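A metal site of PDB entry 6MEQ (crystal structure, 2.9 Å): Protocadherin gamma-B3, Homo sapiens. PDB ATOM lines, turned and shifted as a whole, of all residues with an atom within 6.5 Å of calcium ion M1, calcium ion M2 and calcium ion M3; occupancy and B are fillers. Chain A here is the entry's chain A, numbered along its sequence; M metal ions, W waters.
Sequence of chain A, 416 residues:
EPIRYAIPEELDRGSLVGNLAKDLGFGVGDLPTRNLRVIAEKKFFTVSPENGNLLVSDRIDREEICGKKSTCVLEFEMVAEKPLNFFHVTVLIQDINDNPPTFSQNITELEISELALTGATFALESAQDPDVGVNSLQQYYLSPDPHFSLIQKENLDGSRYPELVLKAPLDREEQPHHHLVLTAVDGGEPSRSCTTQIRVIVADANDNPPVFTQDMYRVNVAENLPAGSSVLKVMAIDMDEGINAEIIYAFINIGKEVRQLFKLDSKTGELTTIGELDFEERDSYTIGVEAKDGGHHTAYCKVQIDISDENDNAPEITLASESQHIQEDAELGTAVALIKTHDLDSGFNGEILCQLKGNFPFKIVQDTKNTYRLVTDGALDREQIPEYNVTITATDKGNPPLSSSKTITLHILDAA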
ATOM      1  N   GLU A 223      21.762  22.907 -13.463  1.00  0.00           N
ATOM      2  CA  GLU A 223      22.889  22.014 -13.201  1.00  0.00           C
ATOM      3  C   GLU A 223      22.421  20.582 -13.029  1.00  0.00           C
ATOM      4  O   GLU A 223      22.882  19.672 -13.732  1.00  0.00           O
ATOM      5  CB  GLU A 223      23.646  22.486 -11.953  1.00  0.00           C
ATOM      6  CG  GLU A 223      24.987  21.801 -11.748  1.00  0.00           C
ATOM      7  CD  GLU A 223      25.567  22.064 -10.376  1.00  0.00           C
ATOM      8  OE1 GLU A 223      25.597  21.116  -9.555  1.00  0.00           O
ATOM      9  OE2 GLU A 223      25.993  23.205 -10.117  1.00  0.00           O
ATOM     10  N   ASN A 224      21.502  20.345 -12.096  1.00  0.00           N
ATOM     11  CA  ASN A 224      20.990  19.002 -11.826  1.00  0.00           C
ATOM     12  C   ASN A 224      19.773  18.701 -12.697  1.00  0.00           C
ATOM     13  O   ASN A 224      18.673  18.408 -12.222  1.00  0.00           O
ATOM     14  CB  ASN A 224      20.678  18.842 -10.340  1.00  0.00           C
ATOM     15  CG  ASN A 224      21.902  18.976  -9.465  1.00  0.00           C
ATOM     16  OD1 ASN A 224      23.015  18.643  -9.873  1.00  0.00           O
ATOM     17  ND2 ASN A 224      21.709  19.475  -8.247  1.00  0.00           N
ATOM     18  N   LEU A 277      24.706  16.365 -15.704  1.00  0.00           N
ATOM     19  CA  LEU A 277      25.408  17.624 -15.861  1.00  0.00           C
ATOM     20  C   LEU A 277      25.991  18.071 -14.519  1.00  0.00           C
ATOM     21  O   LEU A 277      25.453  17.769 -13.461  1.00  0.00           O
ATOM     22  CB  LEU A 277      24.461  18.701 -16.402  1.00  0.00           C
ATOM     23  CG  LEU A 277      23.772  18.408 -17.728  1.00  0.00           C
ATOM     24  CD1 LEU A 277      22.873  19.566 -18.140  1.00  0.00           C
ATOM     25  CD2 LEU A 277      24.798  18.110 -18.812  1.00  0.00           C
ATOM     26  N   ASP A 278      27.107  18.792 -14.592  1.00  0.00           N
ATOM     27  CA  ASP A 278      27.785  19.266 -13.391  1.00  0.00           C
ATOM     28  C   ASP A 278      28.478  20.580 -13.699  1.00  0.00           C
ATOM     29  O   ASP A 278      29.343  20.636 -14.588  1.00  0.00           O
ATOM     30  CB  ASP A 278      28.801  18.224 -12.893  1.00  0.00           C
ATOM     31  CG  ASP A 278      29.329  18.547 -11.504  1.00  0.00           C
ATOM     32  OD1 ASP A 278      28.829  19.504 -10.885  1.00  0.00           O
ATOM     33  OD2 ASP A 278      30.253  17.847 -11.047  1.00  0.00           O
ATOM     34  N   PHE A 279      28.091  21.637 -12.978  1.00  0.00           N
ATOM     35  CA  PHE A 279      28.704  22.946 -13.205  1.00  0.00           C
ATOM     36  C   PHE A 279      30.139  22.990 -12.714  1.00  0.00           C
ATOM     37  O   PHE A 279      30.975  23.693 -13.305  1.00  0.00           O
ATOM     38  CB  PHE A 279      27.865  24.024 -12.517  1.00  0.00           C
ATOM     39  CG  PHE A 279      28.395  25.422 -12.696  1.00  0.00           C
ATOM     40  CD1 PHE A 279      28.048  26.171 -13.802  1.00  0.00           C
ATOM     41  CD2 PHE A 279      29.235  25.984 -11.749  1.00  0.00           C
ATOM     42  CE1 PHE A 279      28.531  27.457 -13.973  1.00  0.00           C
ATOM     43  CE2 PHE A 279      29.726  27.268 -11.913  1.00  0.00           C
ATOM     44  CZ  PHE A 279      29.377  28.004 -13.022  1.00  0.00           C
ATOM     45  N   GLU A 280      30.449  22.264 -11.636  1.00  0.00           N
ATOM     46  CA  GLU A 280      31.809  22.266 -11.099  1.00  0.00           C
ATOM     47  C   GLU A 280      32.808  21.591 -12.021  1.00  0.00           C
ATOM     48  O   GLU A 280      34.010  21.813 -11.884  1.00  0.00           O
ATOM     49  CB  GLU A 280      31.828  21.596  -9.725  1.00  0.00           C
ATOM     50  CG  GLU A 280      31.306  22.463  -8.588  1.00  0.00           C
ATOM     51  CD  GLU A 280      29.816  22.703  -8.664  1.00  0.00           C
ATOM     52  OE1 GLU A 280      29.102  21.867  -9.268  1.00  0.00           O
ATOM     53  OE2 GLU A 280      29.345  23.727  -8.125  1.00  0.00           O
ATOM     54  N   SER A 308      23.908  26.570 -15.590  1.00  0.00           N
ATOM     55  CA  SER A 308      23.880  27.449 -14.429  1.00  0.00           C
ATOM     56  C   SER A 308      24.226  26.667 -13.169  1.00  0.00           C
ATOM     57  O   SER A 308      23.936  25.478 -13.062  1.00  0.00           O
ATOM     58  CB  SER A 308      22.511  28.114 -14.282  1.00  0.00           C
ATOM     59  OG  SER A 308      21.488  27.147 -14.140  1.00  0.00           O
ATOM     60  N   ASP A 309      24.826  27.356 -12.210  1.00  0.00           N
ATOM     61  CA  ASP A 309      25.253  26.720 -10.974  1.00  0.00           C
ATOM     62  C   ASP A 309      24.090  26.556 -10.009  1.00  0.00           C
ATOM     63  O   ASP A 309      23.283  27.477  -9.830  1.00  0.00           O
ATOM     64  CB  ASP A 309      26.369  27.536 -10.306  1.00  0.00           C
ATOM     65  CG  ASP A 309      26.801  26.950  -8.979  1.00  0.00           C
ATOM     66  OD1 ASP A 309      27.372  25.845  -8.972  1.00  0.00           O
ATOM     67  OD2 ASP A 309      26.580  27.610  -7.938  1.00  0.00           O
ATOM     68  N   GLU A 310      24.006  25.381  -9.390  1.00  0.00           N
ATOM     69  CA  GLU A 310      23.011  25.096  -8.377  1.00  0.00           C
ATOM     70  C   GLU A 310      23.698  24.805  -7.049  1.00  0.00           C
ATOM     71  O   GLU A 310      24.809  24.283  -7.012  1.00  0.00           O
ATOM     72  CB  GLU A 310      22.127  23.892  -8.771  1.00  0.00           C
ATOM     73  CG  GLU A 310      21.172  24.169  -9.918  1.00  0.00           C
ATOM     74  CD  GLU A 310      20.017  25.086  -9.522  1.00  0.00           C
ATOM     75  OE1 GLU A 310      19.781  25.243  -8.308  1.00  0.00           O
ATOM     76  OE2 GLU A 310      19.348  25.628 -10.422  1.00  0.00           O
ATOM     77  N   ASN A 311      23.026  25.177  -5.960  1.00  0.00           N
ATOM     78  CA  ASN A 311      23.563  24.979  -4.611  1.00  0.00           C
ATOM     79  C   ASN A 311      23.296  23.534  -4.191  1.00  0.00           C
ATOM     80  O   ASN A 311      22.352  23.224  -3.459  1.00  0.00           O
ATOM     81  CB  ASN A 311      22.955  25.976  -3.636  1.00  0.00           C
ATOM     82  CG  ASN A 311      23.536  25.859  -2.237  1.00  0.00           C
ATOM     83  OD1 ASN A 311      24.652  25.371  -2.065  1.00  0.00           O
ATOM     84  ND2 ASN A 311      22.781  26.300  -1.249  1.00  0.00           N
ATOM     85  N   ASP A 312      24.161  22.633  -4.661  1.00  0.00           N
ATOM     86  CA  ASP A 312      24.057  21.220  -4.333  1.00  0.00           C
ATOM     87  C   ASP A 312      25.292  20.711  -3.587  1.00  0.00           C
ATOM     88  O   ASP A 312      25.441  19.493  -3.432  1.00  0.00           O
ATOM     89  CB  ASP A 312      23.841  20.387  -5.601  1.00  0.00           C
ATOM     90  CG  ASP A 312      25.011  20.479  -6.565  1.00  0.00           C
ATOM     91  OD1 ASP A 312      25.661  21.532  -6.624  1.00  0.00           O
ATOM     92  OD2 ASP A 312      25.275  19.468  -7.265  1.00  0.00           O
ATOM     93  N   ASN A 313      26.152  21.595  -3.116  1.00  0.00           N
ATOM     94  CA  ASN A 313      27.337  21.232  -2.345  1.00  0.00           C
ATOM     95  C   ASN A 313      27.263  21.871  -0.973  1.00  0.00           C
ATOM     96  O   ASN A 313      27.023  23.084  -0.856  1.00  0.00           O
ATOM     97  CB  ASN A 313      28.617  21.660  -3.067  1.00  0.00           C
ATOM     98  CG  ASN A 313      28.943  20.781  -4.257  1.00  0.00           C
ATOM     99  OD1 ASN A 313      29.645  19.786  -4.133  1.00  0.00           O
ATOM    100  ND2 ASN A 313      28.422  21.156  -5.424  1.00  0.00           N
ATOM    101  N   ALA A 314      27.467  21.063   0.066  1.00  0.00           N
ATOM    102  CA  ALA A 314      27.438  21.538   1.445  1.00  0.00           C
ATOM    103  C   ALA A 314      28.810  22.071   1.855  1.00  0.00           C
ATOM    104  O   ALA A 314      29.844  21.600   1.372  1.00  0.00           O
ATOM    105  CB  ALA A 314      27.028  20.419   2.386  1.00  0.00           C
ATOM    106  N   PRO A 315      28.843  23.068   2.735  1.00  0.00           N
ATOM    107  CA  PRO A 315      30.141  23.593   3.202  1.00  0.00           C
ATOM    108  C   PRO A 315      30.916  22.535   3.961  1.00  0.00           C
ATOM    109  O   PRO A 315      30.367  21.737   4.718  1.00  0.00           O
ATOM    110  CB  PRO A 315      29.743  24.757   4.114  1.00  0.00           C
ATOM    111  CG  PRO A 315      28.354  25.138   3.682  1.00  0.00           C
ATOM    112  CD  PRO A 315      27.709  23.853   3.259  1.00  0.00           C
ATOM    113  N   ASP A 343      33.667  25.845  -0.190  1.00  0.00           N
ATOM    114  CA  ASP A 343      32.485  25.294  -0.840  1.00  0.00           C
ATOM    115  C   ASP A 343      32.741  25.202  -2.335  1.00  0.00           C
ATOM    116  O   ASP A 343      33.266  26.139  -2.955  1.00  0.00           O
ATOM    117  CB  ASP A 343      31.249  26.168  -0.568  1.00  0.00           C
ATOM    118  CG  ASP A 343      29.950  25.443  -0.867  1.00  0.00           C
ATOM    119  OD1 ASP A 343      29.528  24.599  -0.054  1.00  0.00           O
ATOM    120  OD2 ASP A 343      29.348  25.717  -1.934  1.00  0.00           O
ATOM    121  N   LEU A 344      32.360  24.066  -2.924  1.00  0.00           N
ATOM    122  CA  LEU A 344      32.630  23.822  -4.336  1.00  0.00           C
ATOM    123  C   LEU A 344      31.776  24.697  -5.246  1.00  0.00           C
ATOM    124  O   LEU A 344      32.139  24.899  -6.410  1.00  0.00           O
ATOM    125  CB  LEU A 344      32.418  22.344  -4.672  1.00  0.00           C
ATOM    126  CG  LEU A 344      33.313  21.354  -3.928  1.00  0.00           C
ATOM    127  CD1 LEU A 344      33.041  19.932  -4.384  1.00  0.00           C
ATOM    128  CD2 LEU A 344      34.783  21.715  -4.112  1.00  0.00           C
ATOM    129  N   ASP A 345      30.655  25.206  -4.758  1.00  0.00           N
ATOM    130  CA  ASP A 345      29.781  26.026  -5.579  1.00  0.00           C
ATOM    131  C   ASP A 345      30.394  27.417  -5.781  1.00  0.00           C
ATOM    132  O   ASP A 345      31.371  27.798  -5.139  1.00  0.00           O
ATOM    133  CB  ASP A 345      28.393  26.144  -4.945  1.00  0.00           C
ATOM    134  CG  ASP A 345      27.771  24.785  -4.674  1.00  0.00           C
ATOM    135  OD1 ASP A 345      27.917  23.884  -5.518  1.00  0.00           O
ATOM    136  OD2 ASP A 345      27.134  24.624  -3.613  1.00  0.00           O
ATOM    137  N   SER A 346      29.786  28.185  -6.689  1.00  0.00           N
ATOM    138  CA  SER A 346      30.252  29.516  -7.035  1.00  0.00           C
ATOM    139  C   SER A 346      29.223  30.554  -6.627  1.00  0.00           C
ATOM    140  O   SER A 346      28.096  30.240  -6.221  1.00  0.00           O
ATOM    141  CB  SER A 346      30.541  29.611  -8.545  1.00  0.00           C
ATOM    142  OG  SER A 346      31.522  28.661  -8.931  1.00  0.00           O
ATOM    143  N   PHE A 348      27.167  33.346  -4.608  1.00  0.00           N
ATOM    144  CA  PHE A 348      26.705  33.357  -3.225  1.00  0.00           C
ATOM    145  C   PHE A 348      26.514  31.946  -2.675  1.00  0.00           C
ATOM    146  O   PHE A 348      26.439  31.774  -1.454  1.00  0.00           O
ATOM    147  CB  PHE A 348      25.398  34.142  -3.101  1.00  0.00           C
ATOM    148  CG  PHE A 348      25.589  35.630  -3.076  1.00  0.00           C
ATOM    149  CD1 PHE A 348      25.837  36.285  -1.886  1.00  0.00           C
ATOM    150  CD2 PHE A 348      25.512  36.366  -4.245  1.00  0.00           C
ATOM    151  CE1 PHE A 348      26.009  37.653  -1.858  1.00  0.00           C
ATOM    152  CE2 PHE A 348      25.689  37.741  -4.220  1.00  0.00           C
ATOM    153  CZ  PHE A 348      25.940  38.387  -3.021  1.00  0.00           C
ATOM    154  N   ASN A 349      26.446  30.937  -3.548  1.00  0.00           N
ATOM    155  CA  ASN A 349      26.342  29.555  -3.098  1.00  0.00           C
ATOM    156  C   ASN A 349      27.647  29.041  -2.505  1.00  0.00           C
ATOM    157  O   ASN A 349      27.637  27.977  -1.864  1.00  0.00           O
ATOM    158  CB  ASN A 349      25.913  28.655  -4.252  1.00  0.00           C
ATOM    159  CG  ASN A 349      24.604  29.096  -4.880  1.00  0.00           C
ATOM    160  OD1 ASN A 349      23.738  29.653  -4.206  1.00  0.00           O
ATOM    161  ND2 ASN A 349      24.456  28.829  -6.171  1.00  0.00           N
ATOM    162  N   GLY A 350      28.757  29.760  -2.685  1.00  0.00           N
ATOM    163  CA  GLY A 350      30.024  29.350  -2.126  1.00  0.00           C
ATOM    164  C   GLY A 350      30.424  30.147  -0.902  1.00  0.00           C
ATOM    165  O   GLY A 350      31.324  29.733  -0.151  1.00  0.00           O
ATOM    166  N   GLU A 351      29.786  31.295  -0.686  1.00  0.00           N
ATOM    167  CA  GLU A 351      30.063  32.108   0.483  1.00  0.00           C
ATOM    168  C   GLU A 351      29.599  31.376   1.739  1.00  0.00           C
ATOM    169  O   GLU A 351      28.426  31.013   1.863  1.00  0.00           O
ATOM    170  CB  GLU A 351      29.356  33.464   0.363  1.00  0.00           C
ATOM    171  CG  GLU A 351      29.676  34.216  -0.918  1.00  0.00           C
ATOM    172  CD  GLU A 351      31.122  34.681  -0.975  1.00  0.00           C
ATOM    173  OE1 GLU A 351      31.733  34.882   0.096  1.00  0.00           O
ATOM    174  OE2 GLU A 351      31.638  34.838  -2.099  1.00  0.00           O
ATOM    175  N   ASP A 396      26.128  28.034   3.968  1.00  0.00           N
ATOM    176  CA  ASP A 396      26.326  28.844   2.774  1.00  0.00           C
ATOM    177  C   ASP A 396      25.175  29.830   2.620  1.00  0.00           C
ATOM    178  O   ASP A 396      24.224  29.853   3.397  1.00  0.00           O
ATOM    179  CB  ASP A 396      26.458  27.944   1.542  1.00  0.00           C
ATOM    180  CG  ASP A 396      25.269  27.031   1.339  1.00  0.00           C
ATOM    181  OD1 ASP A 396      24.201  27.523   0.932  1.00  0.00           O
ATOM    182  OD2 ASP A 396      25.403  25.812   1.593  1.00  0.00           O
ATOM    183  N   LYS A 397      25.265  30.676   1.587  1.00  0.00           N
ATOM    184  CA  LYS A 397      24.267  31.695   1.303  1.00  0.00           C
ATOM    185  C   LYS A 397      23.469  31.359   0.049  1.00  0.00           C
ATOM    186  O   LYS A 397      23.157  32.237  -0.771  1.00  0.00           O
ATOM    187  CB  LYS A 397      24.924  33.073   1.155  1.00  0.00           C
ATOM    188  CG  LYS A 397      25.734  33.509   2.361  1.00  0.00           C
ATOM    189  CD  LYS A 397      26.409  34.844   2.113  1.00  0.00           C
ATOM    190  CE  LYS A 397      27.266  35.263   3.303  1.00  0.00           C
ATOM    191  NZ  LYS A 397      26.460  35.447   4.533  1.00  0.00           N
ATOM    192  N   GLY A 398      23.115  30.085  -0.114  1.00  0.00           N
ATOM    193  CA  GLY A 398      22.374  29.631  -1.265  1.00  0.00           C
ATOM    194  C   GLY A 398      20.871  29.566  -1.014  1.00  0.00           C
ATOM    195  O   GLY A 398      20.373  29.922   0.051  1.00  0.00           O
ATOM    196  N   LEU A 402      22.552  25.152   2.404  1.00  0.00           N
ATOM    197  CA  LEU A 402      23.014  23.917   3.010  1.00  0.00           C
ATOM    198  C   LEU A 402      23.938  24.238   4.184  1.00  0.00           C
ATOM    199  O   LEU A 402      24.442  25.347   4.321  1.00  0.00           O
ATOM    200  CB  LEU A 402      23.736  23.030   1.991  1.00  0.00           C
ATOM    201  CG  LEU A 402      22.897  22.248   0.975  1.00  0.00           C
ATOM    202  CD1 LEU A 402      22.317  23.156  -0.102  1.00  0.00           C
ATOM    203  CD2 LEU A 402      23.734  21.139   0.347  1.00  0.00           C
HETATM  204 CA    CA M   1      26.922  23.299  -7.835  1.00  0.00          CA
HETATM  205 CA    CA M   2      27.039  25.604  -1.058  1.00  0.00          CA
HETATM  206 CA    CA M   3      27.337  19.558  -8.879  1.00  0.00          CA
HETATM  207  O   HOH W   1      27.550  17.654  -6.018  1.00  0.00           O
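Within 4 Å of calcium ion M1: Glu 223, Glu 280, Asp 309, Glu 310, Asp 312, Asn 313 and Asp 345.
Within 4 Å of calcium ion M3: Glu 223, Asp 278, Glu 280, Asp 312 and Asn 313.
The side-chain carboxylate (OD2) of Asp 396 sits at hydrogen-bond distance from the backbone NH (N) of Leu 402, at 3.0 Å.
N of Glu 280 sits close to OD1 of Asp 278, 3.3 Å away.
OD2 of Asp 309 is in hydrogen-bond range of ND2 of Asn 349 (3.0 Å).
The backbone NH (N) of Glu 223 lies close to the backbone carbonyl oxygen (O) of Ser 308, at 3.4 Å.
ND2 of Asn 311 sits at hydrogen-bond distance from OD1 of Asp 396 (2.9 Å).
The backbone NH (N) of Gly 398 lies within hydrogen-bond range of the side-chain carboxylate (OD1) of Asp 396 (3.0 Å).
OD1 of Asp 312 lies close to ND2 of Asn 313 (3.0 Å).
The side-chain carboxylate of Asp 309 is in hydrogen-bond range of the backbone NH of Ser 346.
Calcium ion M3 is bound by the side-chain carboxylate (OE1) of Glu 223 (2.4 Å), the side-chain carboxylate (OD1) of Asp 278 (2.5 Å) and the side-chain carboxylate (OD2) of Asp 312 (2.6 Å).
Slightly farther from calcium ion M3 lies the side-chain carboxylate (OE1) of Glu 280 (2.9 Å).
Calcium ion M2 is bound by OD2 of Asp 343 (2.5 Å), O of Asn 313 (2.5 Å), O of Asn 349 (2.6 Å), OD1 of Asn 311 (2.6 Å), OD2 of Asp 345 (2.7 Å) and OD1 of Asp 343 (2.9 Å).
Slightly farther from calcium ion M2 lies the side-chain carboxylate (OD2) of Asp 396 (3.1 Å).
Calcium ion M1 is bound by the side-chain carboxylate of Glu 223 (2.5 Å), the backbone carbonyl oxygen of Glu 310 (2.5 Å), the side-chain carboxylate of Glu 280 (2.5 Å), the side-chain carboxylate of Asp 312 (2.5 Å), the side-chain carboxylate of Asp 345 (2.6 Å) and the side-chain carboxylate of Asp 309 (2.8 Å).
Slightly farther from calcium ion M1 lies the side-chain carboxylate (OE1) of Glu 280 (3.0 Å).
Slightly farther from calcium ion M1 lies OE1 of Glu 223 (3.1 Å).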
